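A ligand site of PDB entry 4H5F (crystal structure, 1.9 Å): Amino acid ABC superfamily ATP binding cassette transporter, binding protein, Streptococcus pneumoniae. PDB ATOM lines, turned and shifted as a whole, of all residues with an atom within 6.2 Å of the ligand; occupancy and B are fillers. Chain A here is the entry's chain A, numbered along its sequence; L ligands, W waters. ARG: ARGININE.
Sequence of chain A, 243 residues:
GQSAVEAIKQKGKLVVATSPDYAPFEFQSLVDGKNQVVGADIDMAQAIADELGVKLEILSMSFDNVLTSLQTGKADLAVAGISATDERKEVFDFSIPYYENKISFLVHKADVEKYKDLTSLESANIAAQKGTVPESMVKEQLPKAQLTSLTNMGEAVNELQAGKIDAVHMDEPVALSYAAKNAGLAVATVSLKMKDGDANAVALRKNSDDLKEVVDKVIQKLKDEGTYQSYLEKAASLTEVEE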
ATOM      1  N   THR A  18      -9.497  27.569  12.249  1.00  0.00           N
ATOM      2  CA  THR A  18     -10.575  26.649  12.629  1.00  0.00           C
ATOM      3  C   THR A  18     -11.961  27.314  12.591  1.00  0.00           C
ATOM      4  O   THR A  18     -12.084  28.525  12.475  1.00  0.00           O
ATOM      5  CB  THR A  18     -10.351  26.057  14.030  1.00  0.00           C
ATOM      6  OG1 THR A  18     -11.168  24.891  14.175  1.00  0.00           O
ATOM      7  CG2 THR A  18     -10.715  27.058  15.090  1.00  0.00           C
ATOM      8  N   SER A  19     -13.004  26.488  12.709  1.00  0.00           N
ATOM      9  CA  SER A  19     -14.388  26.974  12.735  1.00  0.00           C
ATOM     10  C   SER A  19     -15.095  26.427  13.987  1.00  0.00           C
ATOM     11  O   SER A  19     -15.592  25.295  13.981  1.00  0.00           O
ATOM     12  CB  SER A  19     -15.119  26.514  11.481  1.00  0.00           C
ATOM     13  OG  SER A  19     -16.521  26.636  11.631  1.00  0.00           O
ATOM     14  N   PRO A  20     -15.141  27.230  15.069  1.00  0.00           N
ATOM     15  CA  PRO A  20     -15.561  26.680  16.372  1.00  0.00           C
ATOM     16  C   PRO A  20     -17.068  26.581  16.526  1.00  0.00           C
ATOM     17  O   PRO A  20     -17.593  27.149  17.474  1.00  0.00           O
ATOM     18  CB  PRO A  20     -15.015  27.708  17.366  1.00  0.00           C
ATOM     19  CG  PRO A  20     -14.995  28.995  16.619  1.00  0.00           C
ATOM     20  CD  PRO A  20     -14.705  28.634  15.175  1.00  0.00           C
ATOM     21  N   ASP A  21     -17.723  25.859  15.611  1.00  0.00           N
ATOM     22  CA  ASP A  21     -19.164  25.629  15.666  1.00  0.00           C
ATOM     23  C   ASP A  21     -19.448  24.124  15.625  1.00  0.00           C
ATOM     24  O   ASP A  21     -20.445  23.691  15.041  1.00  0.00           O
ATOM     25  CB  ASP A  21     -19.854  26.324  14.485  1.00  0.00           C
ATOM     26  CG  ASP A  21     -19.382  25.791  13.127  1.00  0.00           C
ATOM     27  OD1 ASP A  21     -18.307  25.149  13.065  1.00  0.00           O
ATOM     28  OD2 ASP A  21     -20.084  26.003  12.117  1.00  0.00           O
ATOM     29  N   TYR A  22     -18.582  23.335  16.252  1.00  0.00           N
ATOM     30  CA  TYR A  22     -18.494  21.913  15.926  1.00  0.00           C
ATOM     31  C   TYR A  22     -18.008  21.033  17.073  1.00  0.00           C
ATOM     32  O   TYR A  22     -17.067  20.247  16.899  1.00  0.00           O
ATOM     33  CB  TYR A  22     -17.535  21.757  14.729  1.00  0.00           C
ATOM     34  CG  TYR A  22     -18.028  20.793  13.679  1.00  0.00           C
ATOM     35  CD1 TYR A  22     -19.298  20.919  13.146  1.00  0.00           C
ATOM     36  CD2 TYR A  22     -17.222  19.772  13.206  1.00  0.00           C
ATOM     37  CE1 TYR A  22     -19.768  20.058  12.196  1.00  0.00           C
ATOM     38  CE2 TYR A  22     -17.686  18.910  12.248  1.00  0.00           C
ATOM     39  CZ  TYR A  22     -18.965  19.069  11.743  1.00  0.00           C
ATOM     40  OH  TYR A  22     -19.427  18.217  10.784  1.00  0.00           O
ATOM     41  N   PHE A  25     -15.108  18.598  18.359  1.00  0.00           N
ATOM     42  CA  PHE A  25     -13.880  18.987  17.673  1.00  0.00           C
ATOM     43  C   PHE A  25     -13.402  20.392  18.081  1.00  0.00           C
ATOM     44  O   PHE A  25     -12.280  20.558  18.569  1.00  0.00           O
ATOM     45  CB  PHE A  25     -14.041  18.884  16.150  1.00  0.00           C
ATOM     46  CG  PHE A  25     -14.245  17.490  15.658  1.00  0.00           C
ATOM     47  CD1 PHE A  25     -13.161  16.650  15.470  1.00  0.00           C
ATOM     48  CD2 PHE A  25     -15.509  17.016  15.393  1.00  0.00           C
ATOM     49  CE1 PHE A  25     -13.353  15.358  15.030  1.00  0.00           C
ATOM     50  CE2 PHE A  25     -15.721  15.746  14.946  1.00  0.00           C
ATOM     51  CZ  PHE A  25     -14.630  14.895  14.765  1.00  0.00           C
ATOM     52  N   GLU A  26     -14.248  21.402  17.869  1.00  0.00           N
ATOM     53  CA  GLU A  26     -13.917  22.770  18.274  1.00  0.00           C
ATOM     54  C   GLU A  26     -15.157  23.577  18.518  1.00  0.00           C
ATOM     55  O   GLU A  26     -16.111  23.502  17.751  1.00  0.00           O
ATOM     56  CB  GLU A  26     -13.035  23.494  17.257  1.00  0.00           C
ATOM     57  CG  GLU A  26     -13.545  23.468  15.833  1.00  0.00           C
ATOM     58  CD  GLU A  26     -12.977  22.303  15.078  1.00  0.00           C
ATOM     59  OE1 GLU A  26     -11.864  21.869  15.409  1.00  0.00           O
ATOM     60  OE2 GLU A  26     -13.641  21.793  14.154  1.00  0.00           O
ATOM     61  N   PHE A  63     -16.447  27.815   8.444  1.00  0.00           N
ATOM     62  CA  PHE A  63     -15.770  26.667   7.809  1.00  0.00           C
ATOM     63  C   PHE A  63     -15.412  26.831   6.329  1.00  0.00           C
ATOM     64  O   PHE A  63     -14.334  26.411   5.895  1.00  0.00           O
ATOM     65  CB  PHE A  63     -16.526  25.347   8.013  1.00  0.00           C
ATOM     66  CG  PHE A  63     -15.791  24.167   7.432  1.00  0.00           C
ATOM     67  CD1 PHE A  63     -14.812  23.524   8.179  1.00  0.00           C
ATOM     68  CD2 PHE A  63     -16.038  23.731   6.142  1.00  0.00           C
ATOM     69  CE1 PHE A  63     -14.113  22.450   7.659  1.00  0.00           C
ATOM     70  CE2 PHE A  63     -15.326  22.656   5.621  1.00  0.00           C
ATOM     71  CZ  PHE A  63     -14.358  22.025   6.382  1.00  0.00           C
ATOM     72  N   ALA A  80      -9.981  21.560  11.628  1.00  0.00           N
ATOM     73  CA  ALA A  80     -11.408  21.847  11.815  1.00  0.00           C
ATOM     74  C   ALA A  80     -12.289  20.633  11.499  1.00  0.00           C
ATOM     75  O   ALA A  80     -13.293  20.756  10.784  1.00  0.00           O
ATOM     76  CB  ALA A  80     -11.814  23.024  10.926  1.00  0.00           C
ATOM     77  N   GLY A  81     -11.914  19.459  12.014  1.00  0.00           N
ATOM     78  CA  GLY A  81     -12.535  18.198  11.610  1.00  0.00           C
ATOM     79  C   GLY A  81     -12.613  18.057  10.097  1.00  0.00           C
ATOM     80  O   GLY A  81     -13.678  17.802   9.537  1.00  0.00           O
ATOM     81  N   ILE A  82     -11.481  18.244   9.419  1.00  0.00           N
ATOM     82  CA  ILE A  82     -11.441  18.337   7.965  1.00  0.00           C
ATOM     83  C   ILE A  82     -11.254  16.953   7.360  1.00  0.00           C
ATOM     84  O   ILE A  82     -10.300  16.252   7.693  1.00  0.00           O
ATOM     85  CB  ILE A  82     -10.311  19.278   7.495  1.00  0.00           C
ATOM     86  CG1 ILE A  82     -10.580  20.695   7.998  1.00  0.00           C
ATOM     87  CG2 ILE A  82     -10.146  19.236   5.967  1.00  0.00           C
ATOM     88  CD1 ILE A  82      -9.353  21.599   7.963  1.00  0.00           C
ATOM     89  N   SER A  83     -12.180  16.560   6.499  1.00  0.00           N
ATOM     90  CA  SER A  83     -12.074  15.297   5.782  1.00  0.00           C
ATOM     91  C   SER A  83     -11.018  15.411   4.716  1.00  0.00           C
ATOM     92  O   SER A  83     -11.037  16.326   3.903  1.00  0.00           O
ATOM     93  CB  SER A  83     -13.402  14.960   5.124  1.00  0.00           C
ATOM     94  OG  SER A  83     -14.452  15.001   6.070  1.00  0.00           O
ATOM     95  N   ALA A  84     -10.089  14.462   4.699  1.00  0.00           N
ATOM     96  CA  ALA A  84      -9.016  14.448   3.730  1.00  0.00           C
ATOM     97  C   ALA A  84      -9.461  13.809   2.427  1.00  0.00           C
ATOM     98  O   ALA A  84      -9.242  12.623   2.223  1.00  0.00           O
ATOM     99  CB  ALA A  84      -7.829  13.718   4.295  1.00  0.00           C
ATOM    100  N   ARG A  88      -9.625  17.604  -2.314  1.00  0.00           N
ATOM    101  CA  ARG A  88      -8.883  18.565  -1.486  1.00  0.00           C
ATOM    102  C   ARG A  88      -7.379  18.364  -1.605  1.00  0.00           C
ATOM    103  O   ARG A  88      -6.608  19.326  -1.511  1.00  0.00           O
ATOM    104  CB  ARG A  88      -9.335  18.478  -0.031  1.00  0.00           C
ATOM    105  CG  ARG A  88     -10.639  19.191   0.235  1.00  0.00           C
ATOM    106  CD  ARG A  88     -11.189  18.868   1.622  1.00  0.00           C
ATOM    107  NE  ARG A  88     -12.419  19.604   1.897  1.00  0.00           N
ATOM    108  CZ  ARG A  88     -13.218  19.366   2.936  1.00  0.00           C
ATOM    109  NH1 ARG A  88     -12.916  18.408   3.787  1.00  0.00           N
ATOM    110  NH2 ARG A  88     -14.322  20.087   3.110  1.00  0.00           N
ATOM    111  N   ILE A 103     -20.708   9.836   9.190  1.00  0.00           N
ATOM    112  CA  ILE A 103     -21.463  11.050   8.990  1.00  0.00           C
ATOM    113  C   ILE A 103     -22.942  10.717   9.145  1.00  0.00           C
ATOM    114  O   ILE A 103     -23.433   9.765   8.548  1.00  0.00           O
ATOM    115  CB  ILE A 103     -21.183  11.669   7.623  1.00  0.00           C
ATOM    116  CG1 ILE A 103     -19.673  11.930   7.491  1.00  0.00           C
ATOM    117  CG2 ILE A 103     -21.952  12.955   7.443  1.00  0.00           C
ATOM    118  CD1 ILE A 103     -19.223  12.252   6.111  1.00  0.00           C
ATOM    119  N   GLN A 129     -23.707  22.011   6.129  1.00  0.00           N
ATOM    120  CA  GLN A 129     -22.825  23.183   6.199  1.00  0.00           C
ATOM    121  C   GLN A 129     -22.196  23.510   4.827  1.00  0.00           C
ATOM    122  O   GLN A 129     -21.706  22.607   4.145  1.00  0.00           O
ATOM    123  CB  GLN A 129     -21.737  22.948   7.254  1.00  0.00           C
ATOM    124  CG  GLN A 129     -20.902  24.179   7.608  1.00  0.00           C
ATOM    125  CD  GLN A 129     -20.153  23.976   8.884  1.00  0.00           C
ATOM    126  OE1 GLN A 129     -19.786  22.854   9.213  1.00  0.00           O
ATOM    127  NE2 GLN A 129     -19.947  25.041   9.645  1.00  0.00           N
ATOM    128  N   GLY A 131     -19.684  24.247   1.977  1.00  0.00           N
ATOM    129  CA  GLY A 131     -18.296  23.890   1.739  1.00  0.00           C
ATOM    130  C   GLY A 131     -17.817  22.603   2.372  1.00  0.00           C
ATOM    131  O   GLY A 131     -16.615  22.379   2.460  1.00  0.00           O
ATOM    132  N   THR A 132     -18.738  21.731   2.803  1.00  0.00           N
ATOM    133  CA  THR A 132     -18.384  20.509   3.506  1.00  0.00           C
ATOM    134  C   THR A 132     -18.724  19.224   2.750  1.00  0.00           C
ATOM    135  O   THR A 132     -19.520  19.218   1.820  1.00  0.00           O
ATOM    136  CB  THR A 132     -19.073  20.450   4.884  1.00  0.00           C
ATOM    137  OG1 THR A 132     -20.488  20.295   4.700  1.00  0.00           O
ATOM    138  CG2 THR A 132     -18.788  21.721   5.688  1.00  0.00           C
ATOM    139  N   VAL A 133     -18.106  18.135   3.173  1.00  0.00           N
ATOM    140  CA  VAL A 133     -18.421  16.800   2.659  1.00  0.00           C
ATOM    141  C   VAL A 133     -19.865  16.352   2.965  1.00  0.00           C
ATOM    142  O   VAL A 133     -20.535  15.852   2.049  1.00  0.00           O
ATOM    143  CB  VAL A 133     -17.395  15.759   3.150  1.00  0.00           C
ATOM    144  CG1 VAL A 133     -17.827  14.352   2.796  1.00  0.00           C
ATOM    145  CG2 VAL A 133     -16.041  16.060   2.545  1.00  0.00           C
ATOM    146  N   PRO A 134     -20.362  16.540   4.213  1.00  0.00           N
ATOM    147  CA  PRO A 134     -21.788  16.276   4.432  1.00  0.00           C
ATOM    148  C   PRO A 134     -22.759  17.008   3.482  1.00  0.00           C
ATOM    149  O   PRO A 134     -23.784  16.426   3.105  1.00  0.00           O
ATOM    150  CB  PRO A 134     -21.984  16.738   5.880  1.00  0.00           C
ATOM    151  CG  PRO A 134     -20.694  16.436   6.533  1.00  0.00           C
ATOM    152  CD  PRO A 134     -19.665  16.774   5.494  1.00  0.00           C
ATOM    153  N   MET A 153     -22.760  25.933  11.586  1.00  0.00           N
ATOM    154  CA  MET A 153     -23.468  24.722  12.030  1.00  0.00           C
ATOM    155  C   MET A 153     -24.508  24.983  13.157  1.00  0.00           C
ATOM    156  O   MET A 153     -25.553  24.335  13.210  1.00  0.00           O
ATOM    157  CB  MET A 153     -22.468  23.628  12.427  1.00  0.00           C
ATOM    158  CG  MET A 153     -23.089  22.288  12.871  1.00  0.00           C
ATOM    159  SD  MET A 153     -24.337  21.618  11.740  1.00  0.00           S
ATOM    160  CE  MET A 153     -23.309  20.988  10.425  1.00  0.00           C
ATOM    161  N   ASP A 171     -20.907  15.554  10.972  1.00  0.00           N
ATOM    162  CA  ASP A 171     -20.050  14.467  11.456  1.00  0.00           C
ATOM    163  C   ASP A 171     -20.721  13.865  12.680  1.00  0.00           C
ATOM    164  O   ASP A 171     -21.300  14.570  13.484  1.00  0.00           O
ATOM    165  CB  ASP A 171     -18.619  14.948  11.759  1.00  0.00           C
ATOM    166  CG  ASP A 171     -17.787  15.081  10.496  1.00  0.00           C
ATOM    167  OD1 ASP A 171     -17.251  14.073   9.999  1.00  0.00           O
ATOM    168  OD2 ASP A 171     -17.668  16.200   9.976  1.00  0.00           O
ATOM    169  N   ASN A 200     -10.541  12.404   9.307  1.00  0.00           N
ATOM    170  CA  ASN A 200     -10.095  13.740   9.670  1.00  0.00           C
ATOM    171  C   ASN A 200      -8.567  13.866   9.677  1.00  0.00           C
ATOM    172  O   ASN A 200      -7.873  12.995  10.192  1.00  0.00           O
ATOM    173  CB  ASN A 200     -10.694  14.143  11.014  1.00  0.00           C
ATOM    174  CG  ASN A 200     -12.193  14.025  11.005  1.00  0.00           C
ATOM    175  OD1 ASN A 200     -12.872  14.752  10.269  1.00  0.00           O
ATOM    176  ND2 ASN A 200     -12.711  13.095  11.779  1.00  0.00           N
HETATM  177  N   ARG L   1     -15.725  16.941   7.989  1.00  0.00           N
HETATM  178  CA  ARG L   1     -16.444  17.866   7.126  1.00  0.00           C
HETATM  179  C   ARG L   1     -15.547  18.425   6.037  1.00  0.00           C
HETATM  180  O   ARG L   1     -16.036  18.992   5.075  1.00  0.00           O
HETATM  181  CB  ARG L   1     -17.068  18.999   7.943  1.00  0.00           C
HETATM  182  CG  ARG L   1     -16.128  19.678   8.925  1.00  0.00           C
HETATM  183  CD  ARG L   1     -16.747  20.978   9.472  1.00  0.00           C
HETATM  184  NE  ARG L   1     -15.940  21.553  10.539  1.00  0.00           N
HETATM  185  CZ  ARG L   1     -16.314  22.579  11.293  1.00  0.00           C
HETATM  186  NH1 ARG L   1     -17.491  23.157  11.088  1.00  0.00           N
HETATM  187  NH2 ARG L   1     -15.511  23.029  12.252  1.00  0.00           N
HETATM  188  OXT ARG L   1     -14.330  18.318   6.084  1.00  0.00           O
HETATM  189  O   HOH W   1     -17.441  14.600   7.172  1.00  0.00           O
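N of the ligand sits at hydrogen-bond distance from OG of Ser 83, 3.0 Å away. OE1 of Gln 129 sits at hydrogen-bond distance from NH1 of the ligand, at 3.0 Å. A nitrogen (N) of the ligand lies within salt-bridge range of the side-chain carboxylate of Asp 171 (2.9 Å). OE2 of Glu 26 is in salt-bridge range of NH2 of the ligand, at 2.9 Å. The backbone NH (N) of Val 133 is in hydrogen-bond range of an oxygen (O) of the ligand, at 2.9 Å. The backbone carbonyl oxygen (O) of Gly 81 is in hydrogen-bond range of a nitrogen (N) of the ligand (2.7 Å). The backbone NH of Ser 83 is in hydrogen-bond range of an oxygen (OXT) of the ligand, at 2.8 Å. OXT of the ligand is in salt-bridge range of NH1 of Arg 88. The backbone carbonyl oxygen (O) of Ala 80 lies within hydrogen-bond range of a nitrogen (NE) of the ligand, 2.8 Å away. The side-chain carboxylate (OD1) of Asp 21 lies within salt-bridge range of a nitrogen (NH1) of the ligand (2.9 Å). A nitrogen (NH2) of the ligand is in hydrogen-bond range of the backbone carbonyl oxygen of Ser 19 (2.9 Å).
NH2 of Arg 88 lies within hydrogen-bond range of O of Gly 131 (3.3 Å). The guanidinium group (NH1) of Arg 88 sits at hydrogen-bond distance from the backbone carbonyl oxygen (O) of Ser 83, at 2.8 Å. OG1 of Thr 132 sits at hydrogen-bond distance from O of Gln 129. The side-chain carboxylate of Asp 21 lies within hydrogen-bond range of the side-chain amide nitrogen of Gln 129 (2.7 Å). The side-chain hydroxyl of Ser 19 sits at hydrogen-bond distance from the backbone NH of Phe 63, at 3.4 Å. OD1 of Asp 21 sits at hydrogen-bond distance from OG of Ser 19. N of Met 153 lies within hydrogen-bond range of OD2 of Asp 21 (2.7 Å). The side-chain carboxylate of Glu 26 sits close to the side-chain hydroxyl of Thr 18 (3.3 Å).
Residues that only touch the ligand: Tyr 22, Phe 63, Ile 82, Thr 132 and Pro 134. Hydrophobic or aromatic side chains that line the ligand: Tyr 22, Phe 63, Ala 80, Val 133 and Pro 134. 15 residues have an atom within 4 Å of the ligand: Ser 19, Asp 21, Tyr 22, Glu 26, Phe 63, Ala 80, Gly 81, Ile 82, Ser 83, Arg 88, Gln 129, Thr 132, Val 133, Pro 134 and Asp 171. Along chain A the residues within 4 Å of the ligand span positions 19 to 171.
Water W1 lies within hydrogen-bond range of the side-chain carboxylate of Asp 171, a nitrogen (N) of the ligand and the side-chain hydroxyl of Ser 83.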
